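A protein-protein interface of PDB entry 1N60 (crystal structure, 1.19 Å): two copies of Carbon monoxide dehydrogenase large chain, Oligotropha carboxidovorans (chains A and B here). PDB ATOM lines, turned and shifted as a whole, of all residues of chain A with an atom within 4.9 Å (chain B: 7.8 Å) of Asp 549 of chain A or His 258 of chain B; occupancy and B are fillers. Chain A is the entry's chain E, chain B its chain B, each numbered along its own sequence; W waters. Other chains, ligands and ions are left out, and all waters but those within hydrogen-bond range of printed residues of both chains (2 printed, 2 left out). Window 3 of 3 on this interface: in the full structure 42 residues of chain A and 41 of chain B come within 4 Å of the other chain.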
ATOM      1  N   GLN A  19      -8.576  31.988 -31.660  1.00  0.00           N
ATOM      2  CA  GLN A  19      -9.410  31.720 -32.824  1.00  0.00           C
ATOM      3  C   GLN A  19     -10.602  32.621 -32.927  1.00  0.00           C
ATOM      4  O   GLN A  19     -11.751  32.192 -33.148  1.00  0.00           O
ATOM      5  CB  GLN A  19      -9.788  30.282 -32.892  1.00  0.00           C
ATOM      6  CG  GLN A  19      -8.566  29.483 -32.984  1.00  0.00           C
ATOM      7  CD  GLN A  19      -8.833  28.141 -33.369  1.00  0.00           C
ATOM      8  OE1 GLN A  19      -9.031  27.911 -34.520  1.00  0.00           O
ATOM      9  NE2 GLN A  19      -8.927  27.225 -32.399  1.00  0.00           N
ATOM     10  N   ARG A  25     -11.146  29.967 -38.639  1.00  0.00           N
ATOM     11  CA  ARG A  25     -11.398  28.936 -37.658  1.00  0.00           C
ATOM     12  C   ARG A  25     -12.099  27.777 -38.348  1.00  0.00           C
ATOM     13  O   ARG A  25     -13.103  27.984 -39.049  1.00  0.00           O
ATOM     14  CB  ARG A  25     -12.247  29.486 -36.528  1.00  0.00           C
ATOM     15  CG  ARG A  25     -12.494  28.469 -35.469  1.00  0.00           C
ATOM     16  CD  ARG A  25     -13.329  28.933 -34.326  1.00  0.00           C
ATOM     17  NE  ARG A  25     -13.450  27.910 -33.334  1.00  0.00           N
ATOM     18  CZ  ARG A  25     -14.504  27.653 -32.596  1.00  0.00           C
ATOM     19  NH1 ARG A  25     -15.630  28.334 -32.711  1.00  0.00           N
ATOM     20  NH2 ARG A  25     -14.415  26.748 -31.653  1.00  0.00           N
ATOM     21  N   VAL A  28     -16.553  23.731 -35.974  1.00  0.00           N
ATOM     22  CA  VAL A  28     -16.849  22.727 -34.968  1.00  0.00           C
ATOM     23  C   VAL A  28     -17.906  21.739 -35.448  1.00  0.00           C
ATOM     24  O   VAL A  28     -17.880  20.593 -35.031  1.00  0.00           O
ATOM     25  CB  VAL A  28     -17.285  23.354 -33.624  1.00  0.00           C
ATOM     26  CG1 VAL A  28     -16.118  24.140 -33.062  1.00  0.00           C
ATOM     27  CG2 VAL A  28     -18.482  24.247 -33.776  1.00  0.00           C
ATOM     28  N   HIS A 514     -19.122  30.250 -17.208  1.00  0.00           N
ATOM     29  CA  HIS A 514     -19.053  29.325 -16.122  1.00  0.00           C
ATOM     30  C   HIS A 514     -17.949  29.689 -15.138  1.00  0.00           C
ATOM     31  O   HIS A 514     -17.034  30.438 -15.476  1.00  0.00           O
ATOM     32  CB  HIS A 514     -18.847  27.911 -16.680  1.00  0.00           C
ATOM     33  CG  HIS A 514     -19.954  27.469 -17.534  1.00  0.00           C
ATOM     34  ND1 HIS A 514     -21.267  27.778 -17.224  1.00  0.00           N
ATOM     35  CD2 HIS A 514     -19.953  26.694 -18.638  1.00  0.00           C
ATOM     36  CE1 HIS A 514     -22.028  27.167 -18.124  1.00  0.00           C
ATOM     37  NE2 HIS A 514     -21.265  26.548 -18.996  1.00  0.00           N
ATOM     38  N   SER A 518     -15.287  28.707 -19.163  1.00  0.00           N
ATOM     39  CA  SER A 518     -15.912  28.301 -20.409  1.00  0.00           C
ATOM     40  C   SER A 518     -17.280  28.908 -20.486  1.00  0.00           C
ATOM     41  O   SER A 518     -17.726  29.548 -19.526  1.00  0.00           O
ATOM     42  CB  SER A 518     -15.905  26.793 -20.501  1.00  0.00           C
ATOM     43  OG  SER A 518     -16.573  26.237 -19.412  1.00  0.00           O
ATOM     44  N   VAL A 519     -17.925  28.777 -21.627  1.00  0.00           N
ATOM     45  CA  VAL A 519     -19.068  29.580 -21.928  1.00  0.00           C
ATOM     46  C   VAL A 519     -20.111  28.782 -22.648  1.00  0.00           C
ATOM     47  O   VAL A 519     -19.762  27.982 -23.524  1.00  0.00           O
ATOM     48  CB  VAL A 519     -18.626  30.705 -22.855  1.00  0.00           C
ATOM     49  CG1 VAL A 519     -19.798  31.599 -23.203  1.00  0.00           C
ATOM     50  CG2 VAL A 519     -17.495  31.503 -22.234  1.00  0.00           C
ATOM     51  N   ILE A 520     -21.388  29.034 -22.334  1.00  0.00           N
ATOM     52  CA  ILE A 520     -22.498  28.595 -23.161  1.00  0.00           C
ATOM     53  C   ILE A 520     -23.171  29.826 -23.674  1.00  0.00           C
ATOM     54  O   ILE A 520     -23.483  30.713 -22.893  1.00  0.00           O
ATOM     55  CB  ILE A 520     -23.488  27.670 -22.402  1.00  0.00           C
ATOM     56  CG1 ILE A 520     -24.689  27.288 -23.261  1.00  0.00           C
ATOM     57  CG2 ILE A 520     -23.962  28.246 -21.070  1.00  0.00           C
ATOM     58  CD1 ILE A 520     -24.365  26.517 -24.453  1.00  0.00           C
ATOM     59  N   PRO A 547     -10.809  31.690 -25.433  1.00  0.00           N
ATOM     60  CA  PRO A 547     -10.633  30.888 -26.650  1.00  0.00           C
ATOM     61  C   PRO A 547     -11.948  30.427 -27.207  1.00  0.00           C
ATOM     62  O   PRO A 547     -12.840  29.981 -26.510  1.00  0.00           O
ATOM     63  CB  PRO A 547      -9.779  29.713 -26.163  1.00  0.00           C
ATOM     64  CG  PRO A 547      -9.057  30.204 -25.011  1.00  0.00           C
ATOM     65  CD  PRO A 547     -10.007  31.183 -24.308  1.00  0.00           C
ATOM     66  N   ALA A 548     -12.050  30.428 -28.530  1.00  0.00           N
ATOM     67  CA  ALA A 548     -13.328  30.015 -29.150  1.00  0.00           C
ATOM     68  C   ALA A 548     -13.726  28.618 -28.780  1.00  0.00           C
ATOM     69  O   ALA A 548     -14.900  28.343 -28.638  1.00  0.00           O
ATOM     70  CB  ALA A 548     -13.237  30.174 -30.623  1.00  0.00           C
ATOM     71  N   ASP A 549     -12.764  27.726 -28.627  1.00  0.00           N
ATOM     72  CA  ASP A 549     -13.076  26.345 -28.248  1.00  0.00           C
ATOM     73  C   ASP A 549     -13.624  26.207 -26.849  1.00  0.00           C
ATOM     74  O   ASP A 549     -14.150  25.163 -26.500  1.00  0.00           O
ATOM     75  CB  ASP A 549     -11.960  25.409 -28.413  1.00  0.00           C
ATOM     76  CG  ASP A 549     -11.750  25.085 -29.860  1.00  0.00           C
ATOM     77  OD1 ASP A 549     -12.754  24.657 -30.582  1.00  0.00           O
ATOM     78  OD2 ASP A 549     -10.595  25.195 -30.295  1.00  0.00           O
ATOM     79  N   ASP A 550     -13.496  27.251 -26.043  1.00  0.00           N
ATOM     80  CA  ASP A 550     -14.023  27.271 -24.696  1.00  0.00           C
ATOM     81  C   ASP A 550     -15.459  27.785 -24.687  1.00  0.00           C
ATOM     82  O   ASP A 550     -16.031  27.974 -23.615  1.00  0.00           O
ATOM     83  CB  ASP A 550     -13.175  28.121 -23.759  1.00  0.00           C
ATOM     84  CG  ASP A 550     -11.852  27.557 -23.504  1.00  0.00           C
ATOM     85  OD1 ASP A 550     -11.465  26.472 -23.989  1.00  0.00           O
ATOM     86  OD2 ASP A 550     -11.085  28.238 -22.813  1.00  0.00           O
ATOM     87  N   ILE A 551     -16.045  27.925 -25.866  1.00  0.00           N
ATOM     88  CA  ILE A 551     -17.369  28.523 -25.973  1.00  0.00           C
ATOM     89  C   ILE A 551     -18.243  27.554 -26.754  1.00  0.00           C
ATOM     90  O   ILE A 551     -17.886  27.148 -27.856  1.00  0.00           O
ATOM     91  CB  ILE A 551     -17.280  29.849 -26.748  1.00  0.00           C
ATOM     92  CG1 ILE A 551     -16.352  30.814 -26.002  1.00  0.00           C
ATOM     93  CG2 ILE A 551     -18.617  30.487 -26.948  1.00  0.00           C
ATOM     94  CD1 ILE A 551     -15.972  32.050 -26.792  1.00  0.00           C
ATOM     95  N   MET A 552     -19.398  27.237 -26.240  1.00  0.00           N
ATOM     96  CA  MET A 552     -20.372  26.410 -26.911  1.00  0.00           C
ATOM     97  C   MET A 552     -21.479  27.272 -27.438  1.00  0.00           C
ATOM     98  O   MET A 552     -22.028  28.022 -26.652  1.00  0.00           O
ATOM     99  CB  MET A 552     -20.962  25.409 -25.903  1.00  0.00           C
ATOM    100  CG  MET A 552     -22.004  24.561 -26.493  1.00  0.00           C
ATOM    101  SD  MET A 552     -21.351  23.383 -27.698  1.00  0.00           S
ATOM    102  CE  MET A 552     -20.191  22.431 -26.702  1.00  0.00           C
ATOM    103  N   GLY B 231     -16.439  14.794 -27.786  1.00  0.00           N
ATOM    104  CA  GLY B 231     -15.674  15.172 -26.612  1.00  0.00           C
ATOM    105  C   GLY B 231     -16.544  15.827 -25.534  1.00  0.00           C
ATOM    106  O   GLY B 231     -16.090  16.713 -24.838  1.00  0.00           O
ATOM    107  N   GLU B 232     -17.787  15.380 -25.398  1.00  0.00           N
ATOM    108  CA  GLU B 232     -18.720  15.961 -24.450  1.00  0.00           C
ATOM    109  C   GLU B 232     -19.320  14.896 -23.593  1.00  0.00           C
ATOM    110  O   GLU B 232     -19.756  13.836 -24.068  1.00  0.00           O
ATOM    111  CB  GLU B 232     -19.839  16.647 -25.144  1.00  0.00           C
ATOM    112  CG  GLU B 232     -19.405  17.824 -25.978  1.00  0.00           C
ATOM    113  CD  GLU B 232     -20.484  18.452 -26.791  1.00  0.00           C
ATOM    114  OE1 GLU B 232     -21.649  18.470 -26.301  1.00  0.00           O
ATOM    115  OE2 GLU B 232     -20.142  19.053 -27.821  1.00  0.00           O
ATOM    116  N   LEU B 233     -19.354  15.183 -22.289  1.00  0.00           N
ATOM    117  CA  LEU B 233     -19.901  14.253 -21.338  1.00  0.00           C
ATOM    118  C   LEU B 233     -21.276  14.677 -20.953  1.00  0.00           C
ATOM    119  O   LEU B 233     -21.481  15.811 -20.537  1.00  0.00           O
ATOM    120  CB  LEU B 233     -18.999  14.257 -20.092  1.00  0.00           C
ATOM    121  CG  LEU B 233     -19.445  13.422 -18.906  1.00  0.00           C
ATOM    122  CD1 LEU B 233     -19.466  11.984 -19.207  1.00  0.00           C
ATOM    123  CD2 LEU B 233     -18.593  13.707 -17.669  1.00  0.00           C
ATOM    124  N   ARG B 246     -21.247  19.507 -11.771  1.00  0.00           N
ATOM    125  CA  ARG B 246     -20.566  19.833 -13.015  1.00  0.00           C
ATOM    126  C   ARG B 246     -19.177  20.395 -12.783  1.00  0.00           C
ATOM    127  O   ARG B 246     -18.190  19.995 -13.403  1.00  0.00           O
ATOM    128  CB  ARG B 246     -21.385  20.791 -13.897  1.00  0.00           C
ATOM    129  CG  ARG B 246     -20.749  20.996 -15.222  1.00  0.00           C
ATOM    130  CD  ARG B 246     -21.397  22.056 -16.031  1.00  0.00           C
ATOM    131  NE  ARG B 246     -21.149  23.356 -15.444  1.00  0.00           N
ATOM    132  CZ  ARG B 246     -21.893  24.443 -15.648  1.00  0.00           C
ATOM    133  NH1 ARG B 246     -22.949  24.459 -16.433  1.00  0.00           N
ATOM    134  NH2 ARG B 246     -21.544  25.522 -15.018  1.00  0.00           N
ATOM    135  N   SER B 250     -15.687  18.714 -13.793  1.00  0.00           N
ATOM    136  CA  SER B 250     -14.752  19.430 -14.636  1.00  0.00           C
ATOM    137  C   SER B 250     -13.371  19.459 -14.010  1.00  0.00           C
ATOM    138  O   SER B 250     -12.377  19.192 -14.638  1.00  0.00           O
ATOM    139  CB  SER B 250     -15.239  20.844 -14.852  1.00  0.00           C
ATOM    140  OG  SER B 250     -14.335  21.563 -15.670  1.00  0.00           O
ATOM    141  N   LEU B 255     -12.311  17.950 -18.334  1.00  0.00           N
ATOM    142  CA  LEU B 255     -13.200  18.416 -19.376  1.00  0.00           C
ATOM    143  C   LEU B 255     -13.721  19.735 -18.948  1.00  0.00           C
ATOM    144  O   LEU B 255     -14.025  19.951 -17.768  1.00  0.00           O
ATOM    145  CB  LEU B 255     -14.375  17.485 -19.529  1.00  0.00           C
ATOM    146  CG  LEU B 255     -14.020  16.134 -20.087  1.00  0.00           C
ATOM    147  CD1 LEU B 255     -15.261  15.218 -19.933  1.00  0.00           C
ATOM    148  CD2 LEU B 255     -13.555  16.228 -21.578  1.00  0.00           C
ATOM    149  N   PRO B 256     -13.882  20.652 -19.862  1.00  0.00           N
ATOM    150  CA  PRO B 256     -14.402  21.978 -19.542  1.00  0.00           C
ATOM    151  C   PRO B 256     -15.884  21.936 -19.309  1.00  0.00           C
ATOM    152  O   PRO B 256     -16.567  21.060 -19.818  1.00  0.00           O
ATOM    153  CB  PRO B 256     -14.005  22.800 -20.753  1.00  0.00           C
ATOM    154  CG  PRO B 256     -14.093  21.772 -21.900  1.00  0.00           C
ATOM    155  CD  PRO B 256     -13.580  20.500 -21.285  1.00  0.00           C
ATOM    156  N   GLU B 257     -16.354  22.887 -18.517  1.00  0.00           N
ATOM    157  CA  GLU B 257     -17.723  22.883 -18.100  1.00  0.00           C
ATOM    158  C   GLU B 257     -18.744  22.951 -19.199  1.00  0.00           C
ATOM    159  O   GLU B 257     -19.850  22.424 -19.083  1.00  0.00           O
ATOM    160  CB  GLU B 257     -17.960  23.991 -17.052  1.00  0.00           C
ATOM    161  CG  GLU B 257     -17.350  23.709 -15.704  1.00  0.00           C
ATOM    162  CD  GLU B 257     -17.828  24.715 -14.709  1.00  0.00           C
ATOM    163  OE1 GLU B 257     -18.926  24.545 -14.154  1.00  0.00           O
ATOM    164  OE2 GLU B 257     -17.057  25.698 -14.514  1.00  0.00           O
ATOM    165  N   HIS B 258     -18.450  23.654 -20.277  1.00  0.00           N
ATOM    166  CA  HIS B 258     -19.352  23.751 -21.397  1.00  0.00           C
ATOM    167  C   HIS B 258     -19.466  22.451 -22.161  1.00  0.00           C
ATOM    168  O   HIS B 258     -20.364  22.298 -23.001  1.00  0.00           O
ATOM    169  CB  HIS B 258     -18.999  24.865 -22.377  1.00  0.00           C
ATOM    170  CG  HIS B 258     -17.699  24.665 -23.049  1.00  0.00           C
ATOM    171  ND1 HIS B 258     -17.437  24.875 -24.395  1.00  0.00           N
ATOM    172  CD2 HIS B 258     -16.541  24.282 -22.492  1.00  0.00           C
ATOM    173  CE1 HIS B 258     -16.158  24.582 -24.617  1.00  0.00           C
ATOM    174  NE2 HIS B 258     -15.607  24.236 -23.477  1.00  0.00           N
ATOM    175  N   LYS B 259     -18.631  21.492 -21.860  1.00  0.00           N
ATOM    176  CA  LYS B 259     -18.697  20.167 -22.479  1.00  0.00           C
ATOM    177  C   LYS B 259     -19.096  19.073 -21.498  1.00  0.00           C
ATOM    178  O   LYS B 259     -18.920  17.900 -21.777  1.00  0.00           O
ATOM    179  CB  LYS B 259     -17.393  19.885 -23.205  1.00  0.00           C
ATOM    180  CG  LYS B 259     -17.187  20.837 -24.368  1.00  0.00           C
ATOM    181  CD  LYS B 259     -16.060  20.518 -25.230  1.00  0.00           C
ATOM    182  CE  LYS B 259     -15.981  21.458 -26.443  1.00  0.00           C
ATOM    183  NZ  LYS B 259     -14.761  21.275 -27.238  1.00  0.00           N
ATOM    184  N   ILE B 260     -19.614  19.506 -20.360  1.00  0.00           N
ATOM    185  CA  ILE B 260     -20.148  18.598 -19.374  1.00  0.00           C
ATOM    186  C   ILE B 260     -21.598  19.004 -19.131  1.00  0.00           C
ATOM    187  O   ILE B 260     -21.884  20.078 -18.669  1.00  0.00           O
ATOM    188  CB  ILE B 260     -19.402  18.648 -18.047  1.00  0.00           C
ATOM    189  CG1 ILE B 260     -17.965  18.319 -18.229  1.00  0.00           C
ATOM    190  CG2 ILE B 260     -20.075  17.690 -17.059  1.00  0.00           C
ATOM    191  CD1 ILE B 260     -17.142  18.630 -17.043  1.00  0.00           C
ATOM    192  N   HIS B 261     -22.509  18.149 -19.542  1.00  0.00           N
ATOM    193  CA  HIS B 261     -23.919  18.396 -19.490  1.00  0.00           C
ATOM    194  C   HIS B 261     -24.512  17.557 -18.403  1.00  0.00           C
ATOM    195  O   HIS B 261     -24.795  16.396 -18.574  1.00  0.00           O
ATOM    196  CB  HIS B 261     -24.553  18.012 -20.841  1.00  0.00           C
ATOM    197  CG  HIS B 261     -23.787  18.542 -21.998  1.00  0.00           C
ATOM    198  ND1 HIS B 261     -23.533  19.881 -22.183  1.00  0.00           N
ATOM    199  CD2 HIS B 261     -23.192  17.897 -23.033  1.00  0.00           C
ATOM    200  CE1 HIS B 261     -22.780  20.043 -23.252  1.00  0.00           C
ATOM    201  NE2 HIS B 261     -22.590  18.859 -23.804  1.00  0.00           N
ATOM    202  N   ASP B 559     -26.844  22.887 -18.485  1.00  0.00           N
ATOM    203  CA  ASP B 559     -26.704  23.654 -19.694  1.00  0.00           C
ATOM    204  C   ASP B 559     -27.698  24.795 -19.743  1.00  0.00           C
ATOM    205  O   ASP B 559     -27.456  25.766 -20.410  1.00  0.00           O
ATOM    206  CB  ASP B 559     -27.039  22.777 -20.914  1.00  0.00           C
ATOM    207  CG  ASP B 559     -25.995  21.816 -21.305  1.00  0.00           C
ATOM    208  OD1 ASP B 559     -24.889  21.758 -20.789  1.00  0.00           O
ATOM    209  OD2 ASP B 559     -26.249  21.089 -22.292  1.00  0.00           O
HETATM  210  O   HOH W   1     -14.531  25.070 -18.038  1.00  0.00           O
HETATM  211  O   HOH W   2     -15.081  23.254 -29.252  1.00  0.00           O
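The backbone NH of Glu 257 of chain B is in hydrogen-bond range of the side-chain hydroxyl of Ser 518 of chain A, at 3.5 Å.
A ring nitrogen (ND1) of His 258 of chain B lies within hydrogen-bond range of the backbone carbonyl oxygen (O) of Asp 550 of chain A, 3.5 Å away.
O of Asp 549 of chain A lies close to NE2 of His 258 of chain B (3.5 Å).
N of His 258 of chain B is in hydrogen-bond range of OG of Ser 518 of chain A (3.3 Å).
NH2 of Arg 246 of chain B sits at hydrogen-bond distance from ND1 of His 514 of chain A (3.2 Å).
Among the printed residues, merely in contact across the chains: Val 519 of chain A with His 258 of chain B, Met 552 of chain A with Glu 232 of chain B, Ile 551 of chain A with His 258 of chain B, His 514 of chain A with Glu 257 of chain B, Met 552 of chain A with His 258 of chain B and His 514 of chain A with His 258 of chain B.
Water W1 bridges OG of Ser 518 of chain A (2.7 Å) and N of Glu 257 of chain B (2.9 Å).
Water W2 bridges the side-chain amino group (NZ) of Lys 259 of chain B (2.8 Å) and the side-chain carboxylate (OD1) of Asp 549 of chain A (3.0 Å).
Printed residues of chain A that touch a printed residue of chain B: His 514, Ser 518, Val 519, Asp 549, Asp 550, Ile 551 and Met 552.
Of the 13 printed residues of chain B, 4 touch a printed residue of chain A.
Printed residues of chain B that touch a printed residue of chain A: Glu 232, Arg 246, Glu 257 and His 258.
Hydrophobic or aromatic side chains of chain B within 4 Å of the printed part of chain A: His 258.
Among the printed residues, 11 pairs touch across the chains.
Among the printed residues, no Asp or Glu carboxylate lies within 4 Å of a Lys or Arg side-chain nitrogen of the other chain.
The backbone carbonyl oxygen (O) of Val 519 of chain A lies within hydrogen-bond range of the backbone NH (N) of Met 552 of chain A.
The backbone carbonyl oxygen of Asp 550 of chain A sits at hydrogen-bond distance from the backbone NH of Val 519 of chain A (2.9 Å).
The side-chain carboxylate (OE1) of Glu 232 of chain B lies within hydrogen-bond range of a ring nitrogen (NE2) of His 261 of chain B.
The side-chain amide nitrogen (NE2) of Gln 19 of chain A lies within hydrogen-bond range of the side-chain carboxylate (OD2) of Asp 549 of chain A, 3.4 Å away.
NE of Arg 246 of chain B lies within salt-bridge range of OE1 of Glu 257 of chain B, at 2.8 Å.
NH2 of Arg 25 of chain A lies within salt-bridge range of OD1 of Asp 549 of chain A, at 2.9 Å.
No position is printed for both chains.
Of the printed residues of chain B, Asp 549 of chain A touches His 258 (2.8 Å).
Of chain A, only His 514 (3.8 Å), Ser 518 (3.3 Å), Val 519 (3.4 Å), Asp 549 (2.8 Å), Asp 550 (3.3 Å), Ile 551 (3.6 Å) and Met 552 (3.6 Å) come within 4 Å of His 258 of chain B.
Ala 548 of chain A touches none of the printed residues of chain B.
Printed residues of chain B within 4 Å of Met 552 of chain A: Glu 232 (3.6 Å) and His 258 (3.6 Å).
Printed residues of chain B within 4 Å of Asp 550 of chain A: His 258.
Printed residues of chain B within 4 Å of His 514 of chain A: Arg 246, Glu 257 and His 258.
Of the printed residues of chain B, Ser 518 of chain A touches Glu 257 (3.5 Å) and His 258 (3.3 Å).
Ser 250 of chain B touches none of the printed residues of chain A.
The nearest printed residue of chain B that does not touch Asp 549 of chain A is Lys 259 of chain B (4.004 Å).
The nearest residue of chain A that does not touch His 258 of chain B is Ile 520 of chain A (4.8 Å).
The nearest printed residue of chain B that does not touch Met 552 of chain A is Lys 259 of chain B (4.1 Å).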
